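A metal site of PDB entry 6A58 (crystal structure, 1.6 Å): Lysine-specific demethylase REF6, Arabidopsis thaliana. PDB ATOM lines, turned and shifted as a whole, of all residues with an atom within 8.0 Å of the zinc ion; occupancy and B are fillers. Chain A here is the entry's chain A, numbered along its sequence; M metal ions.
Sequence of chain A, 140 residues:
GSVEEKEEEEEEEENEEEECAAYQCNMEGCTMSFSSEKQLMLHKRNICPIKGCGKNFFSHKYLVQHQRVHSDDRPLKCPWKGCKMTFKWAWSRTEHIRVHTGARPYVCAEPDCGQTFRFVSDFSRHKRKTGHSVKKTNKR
Of the 18 residues printed, 4 come within 4 Å of the zinc ion.
NE2 of His 43 is bound to the zinc ion (2.1 Å). NE2 of His 60 binds the zinc ion (2.2 Å). The zinc ion is bound by SG of Cys 30, at 2.3 Å. The zinc ion is bound by SG of Cys 25 (2.3 Å). The zinc ion has four donor atoms within binding distance.
SG of Cys 30 lies close to N of Met 32, 3.6 Å away. SG of Cys 25 sits close to N of Met 27, 3.5 Å away. N of Cys 25 sits at hydrogen-bond distance from O of Met 32, 3.1 Å away. The backbone NH of His 60 sits close to the side-chain amide nitrogen of Asn 46.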
ATOM      1  N   GLN A  24     -20.223  -2.744   7.499  1.00  0.00           N
ATOM      2  CA  GLN A  24     -19.617  -2.223   6.269  1.00  0.00           C
ATOM      3  C   GLN A  24     -18.103  -2.470   6.257  1.00  0.00           C
ATOM      4  O   GLN A  24     -17.443  -2.422   7.304  1.00  0.00           O
ATOM      5  CB  GLN A  24     -19.924  -0.722   6.121  1.00  0.00           C
ATOM      6  CG  GLN A  24     -21.389  -0.380   5.870  1.00  0.00           C
ATOM      7  CD  GLN A  24     -22.280  -0.396   7.105  1.00  0.00           C
ATOM      8  OE1 GLN A  24     -21.795  -0.365   8.241  1.00  0.00           O
ATOM      9  NE2 GLN A  24     -23.593  -0.429   6.895  1.00  0.00           N
ATOM     10  N   CYS A  25     -17.567  -2.744   5.076  1.00  0.00           N
ATOM     11  CA  CYS A  25     -16.126  -2.916   4.888  1.00  0.00           C
ATOM     12  C   CYS A  25     -15.437  -1.558   4.814  1.00  0.00           C
ATOM     13  O   CYS A  25     -15.882  -0.679   4.092  1.00  0.00           O
ATOM     14  CB  CYS A  25     -15.813  -3.701   3.617  1.00  0.00           C
ATOM     15  SG  CYS A  25     -14.043  -4.016   3.385  1.00  0.00           S
ATOM     16  N   ASN A  26     -14.333  -1.410   5.560  1.00  0.00           N
ATOM     17  CA  ASN A  26     -13.586  -0.145   5.601  1.00  0.00           C
ATOM     18  C   ASN A  26     -12.370  -0.080   4.660  1.00  0.00           C
ATOM     19  O   ASN A  26     -11.609   0.887   4.717  1.00  0.00           O
ATOM     20  CB  ASN A  26     -13.168   0.200   7.050  1.00  0.00           C
ATOM     21  CG  ASN A  26     -12.195  -0.799   7.645  1.00  0.00           C
ATOM     22  OD1 ASN A  26     -11.870  -1.836   7.053  1.00  0.00           O
ATOM     23  ND2 ASN A  26     -11.733  -0.492   8.864  1.00  0.00           N
ATOM     24  N   MET A  27     -12.201  -1.092   3.817  1.00  0.00           N
ATOM     25  CA  MET A  27     -11.116  -1.089   2.822  1.00  0.00           C
ATOM     26  C   MET A  27     -11.409  -0.060   1.738  1.00  0.00           C
ATOM     27  O   MET A  27     -12.554   0.108   1.324  1.00  0.00           O
ATOM     28  CB  MET A  27     -10.940  -2.473   2.200  1.00  0.00           C
ATOM     29  CG  MET A  27     -10.477  -3.542   3.181  1.00  0.00           C
ATOM     30  SD  MET A  27      -8.781  -3.295   3.734  1.00  0.00           S
ATOM     31  CE  MET A  27      -7.879  -3.782   2.271  1.00  0.00           C
ATOM     32  N   GLU A  28     -10.358   0.629   1.287  1.00  0.00           N
ATOM     33  CA  GLU A  28     -10.504   1.718   0.328  1.00  0.00           C
ATOM     34  C   GLU A  28     -11.145   1.214  -0.973  1.00  0.00           C
ATOM     35  O   GLU A  28     -10.690   0.222  -1.544  1.00  0.00           O
ATOM     36  CB  GLU A  28      -9.142   2.370   0.026  1.00  0.00           C
ATOM     37  CG  GLU A  28      -9.231   3.729  -0.679  1.00  0.00           C
ATOM     38  CD  GLU A  28      -9.827   4.825   0.192  1.00  0.00           C
ATOM     39  OE1 GLU A  28     -10.647   5.611  -0.334  1.00  0.00           O
ATOM     40  OE2 GLU A  28      -9.490   4.904   1.393  1.00  0.00           O
ATOM     41  N   GLY A  29     -12.212   1.883  -1.402  1.00  0.00           N
ATOM     42  CA  GLY A  29     -12.927   1.535  -2.621  1.00  0.00           C
ATOM     43  C   GLY A  29     -13.982   0.451  -2.486  1.00  0.00           C
ATOM     44  O   GLY A  29     -14.757   0.247  -3.422  1.00  0.00           O
ATOM     45  N   CYS A  30     -14.041  -0.244  -1.349  1.00  0.00           N
ATOM     46  CA  CYS A  30     -14.989  -1.342  -1.175  1.00  0.00           C
ATOM     47  C   CYS A  30     -16.363  -0.813  -0.780  1.00  0.00           C
ATOM     48  O   CYS A  30     -16.466   0.086   0.067  1.00  0.00           O
ATOM     49  CB  CYS A  30     -14.505  -2.335  -0.119  1.00  0.00           C
ATOM     50  SG  CYS A  30     -15.446  -3.892  -0.146  1.00  0.00           S
ATOM     51  N   THR A  31     -17.414  -1.365  -1.372  1.00  0.00           N
ATOM     52  CA  THR A  31     -18.787  -0.963  -1.091  1.00  0.00           C
ATOM     53  C   THR A  31     -19.615  -2.121  -0.523  1.00  0.00           C
ATOM     54  O   THR A  31     -20.841  -2.033  -0.472  1.00  0.00           O
ATOM     55  CB  THR A  31     -19.475  -0.397  -2.359  1.00  0.00           C
ATOM     56  OG1 THR A  31     -19.569  -1.415  -3.346  1.00  0.00           O
ATOM     57  CG2 THR A  31     -18.696   0.793  -2.911  1.00  0.00           C
ATOM     58  N   MET A  32     -18.944  -3.178  -0.074  1.00  0.00           N
ATOM     59  CA  MET A  32     -19.634  -4.365   0.429  1.00  0.00           C
ATOM     60  C   MET A  32     -20.013  -4.246   1.900  1.00  0.00           C
ATOM     61  O   MET A  32     -19.361  -3.529   2.671  1.00  0.00           O
ATOM     62  CB  MET A  32     -18.784  -5.618   0.223  1.00  0.00           C
ATOM     63  CG  MET A  32     -18.578  -5.947  -1.246  1.00  0.00           C
ATOM     64  SD  MET A  32     -17.684  -7.499  -1.432  1.00  0.00           S
ATOM     65  CE  MET A  32     -17.452  -7.537  -3.200  1.00  0.00           C
ATOM     66  N   SER A  33     -21.079  -4.933   2.279  1.00  0.00           N
ATOM     67  CA  SER A  33     -21.517  -5.015   3.678  1.00  0.00           C
ATOM     68  C   SER A  33     -22.043  -6.414   3.989  1.00  0.00           C
ATOM     69  O   SER A  33     -22.344  -7.183   3.076  1.00  0.00           O
ATOM     70  CB  SER A  33     -22.583  -3.964   3.976  1.00  0.00           C
ATOM     71  OG  SER A  33     -23.781  -4.256   3.290  1.00  0.00           O
ATOM     72  N   PHE A  34     -22.136  -6.712   5.279  1.00  0.00           N
ATOM     73  CA  PHE A  34     -22.362  -8.077   5.788  1.00  0.00           C
ATOM     74  C   PHE A  34     -23.372  -8.121   6.916  1.00  0.00           C
ATOM     75  O   PHE A  34     -23.536  -7.145   7.645  1.00  0.00           O
ATOM     76  CB  PHE A  34     -21.012  -8.686   6.210  1.00  0.00           C
ATOM     77  CG  PHE A  34     -20.027  -8.698   5.086  1.00  0.00           C
ATOM     78  CD1 PHE A  34     -20.000  -9.751   4.189  1.00  0.00           C
ATOM     79  CD2 PHE A  34     -19.220  -7.578   4.844  1.00  0.00           C
ATOM     80  CE1 PHE A  34     -19.145  -9.732   3.108  1.00  0.00           C
ATOM     81  CE2 PHE A  34     -18.371  -7.561   3.755  1.00  0.00           C
ATOM     82  CZ  PHE A  34     -18.337  -8.634   2.889  1.00  0.00           C
ATOM     83  N   LEU A  40     -17.871 -10.110   8.093  1.00  0.00           N
ATOM     84  CA  LEU A  40     -16.963  -8.989   7.805  1.00  0.00           C
ATOM     85  C   LEU A  40     -15.504  -9.389   8.073  1.00  0.00           C
ATOM     86  O   LEU A  40     -14.624  -9.048   7.292  1.00  0.00           O
ATOM     87  CB  LEU A  40     -17.334  -7.755   8.618  1.00  0.00           C
ATOM     88  CG  LEU A  40     -16.381  -6.561   8.468  1.00  0.00           C
ATOM     89  CD1 LEU A  40     -16.359  -6.069   7.033  1.00  0.00           C
ATOM     90  CD2 LEU A  40     -16.754  -5.431   9.425  1.00  0.00           C
ATOM     91  N   HIS A  43     -14.412 -11.623   5.352  1.00  0.00           N
ATOM     92  CA  HIS A  43     -14.211 -10.757   4.201  1.00  0.00           C
ATOM     93  C   HIS A  43     -12.845 -10.043   4.217  1.00  0.00           C
ATOM     94  O   HIS A  43     -12.183  -9.956   3.190  1.00  0.00           O
ATOM     95  CB  HIS A  43     -15.341  -9.737   4.109  1.00  0.00           C
ATOM     96  CG  HIS A  43     -15.172  -8.737   3.012  1.00  0.00           C
ATOM     97  ND1 HIS A  43     -15.291  -9.071   1.673  1.00  0.00           N
ATOM     98  CD2 HIS A  43     -14.907  -7.409   3.040  1.00  0.00           C
ATOM     99  CE1 HIS A  43     -15.104  -7.996   0.933  1.00  0.00           C
ATOM    100  NE2 HIS A  43     -14.855  -6.973   1.742  1.00  0.00           N
ATOM    101  N   LYS A  44     -12.439  -9.556   5.395  1.00  0.00           N
ATOM    102  CA  LYS A  44     -11.126  -8.902   5.537  1.00  0.00           C
ATOM    103  C   LYS A  44      -9.933  -9.862   5.383  1.00  0.00           C
ATOM    104  O   LYS A  44      -8.808  -9.407   5.148  1.00  0.00           O
ATOM    105  CB  LYS A  44     -11.048  -8.125   6.863  1.00  0.00           C
ATOM    106  CG  LYS A  44     -11.921  -6.890   6.846  1.00  0.00           C
ATOM    107  CD  LYS A  44     -11.946  -6.203   8.187  1.00  0.00           C
ATOM    108  CE  LYS A  44     -12.865  -4.989   8.150  1.00  0.00           C
ATOM    109  NZ  LYS A  44     -12.875  -4.250   9.429  1.00  0.00           N
ATOM    110  N   ASN A  46     -10.001 -11.879   2.907  1.00  0.00           N
ATOM    111  CA  ASN A  46     -10.135 -12.115   1.471  1.00  0.00           C
ATOM    112  C   ASN A  46     -10.717 -13.474   1.092  1.00  0.00           C
ATOM    113  O   ASN A  46     -10.317 -14.087   0.102  1.00  0.00           O
ATOM    114  CB  ASN A  46      -8.785 -11.860   0.765  1.00  0.00           C
ATOM    115  CG  ASN A  46      -8.274 -10.444   1.015  1.00  0.00           C
ATOM    116  OD1 ASN A  46      -7.117 -10.245   1.373  1.00  0.00           O
ATOM    117  ND2 ASN A  46      -9.141  -9.471   0.840  1.00  0.00           N
ATOM    118  N   HIS A  60      -7.308  -7.740  -1.561  1.00  0.00           N
ATOM    119  CA  HIS A  60      -8.701  -7.328  -1.599  1.00  0.00           C
ATOM    120  C   HIS A  60      -9.180  -7.047  -3.025  1.00  0.00           C
ATOM    121  O   HIS A  60     -10.349  -7.279  -3.331  1.00  0.00           O
ATOM    122  CB  HIS A  60      -8.883  -6.109  -0.694  1.00  0.00           C
ATOM    123  CG  HIS A  60     -10.296  -5.869  -0.323  1.00  0.00           C
ATOM    124  ND1 HIS A  60     -11.149  -5.136  -1.116  1.00  0.00           N
ATOM    125  CD2 HIS A  60     -11.031  -6.287   0.740  1.00  0.00           C
ATOM    126  CE1 HIS A  60     -12.338  -5.093  -0.550  1.00  0.00           C
ATOM    127  NE2 HIS A  60     -12.300  -5.779   0.581  1.00  0.00           N
ATOM    128  N   LEU A  63     -10.133 -10.399  -4.601  1.00  0.00           N
ATOM    129  CA  LEU A  63     -11.403 -10.833  -4.013  1.00  0.00           C
ATOM    130  C   LEU A  63     -12.613 -10.194  -4.708  1.00  0.00           C
ATOM    131  O   LEU A  63     -13.558 -10.892  -5.081  1.00  0.00           O
ATOM    132  CB  LEU A  63     -11.437 -10.504  -2.526  1.00  0.00           C
ATOM    133  CG  LEU A  63     -12.732 -10.791  -1.756  1.00  0.00           C
ATOM    134  CD1 LEU A  63     -12.925 -12.286  -1.596  1.00  0.00           C
ATOM    135  CD2 LEU A  63     -12.728 -10.063  -0.416  1.00  0.00           C
ATOM    136  N   VAL A  64     -12.573  -8.870  -4.844  1.00  0.00           N
ATOM    137  CA  VAL A  64     -13.698  -8.105  -5.402  1.00  0.00           C
ATOM    138  C   VAL A  64     -13.952  -8.470  -6.875  1.00  0.00           C
ATOM    139  O   VAL A  64     -15.096  -8.636  -7.286  1.00  0.00           O
ATOM    140  CB  VAL A  64     -13.469  -6.574  -5.248  1.00  0.00           C
ATOM    141  CG1 VAL A  64     -14.505  -5.761  -6.028  1.00  0.00           C
ATOM    142  CG2 VAL A  64     -13.515  -6.178  -3.779  1.00  0.00           C
HETATM  143 ZN    ZN M   1     -14.200  -5.038   1.343  1.00  0.00          ZN
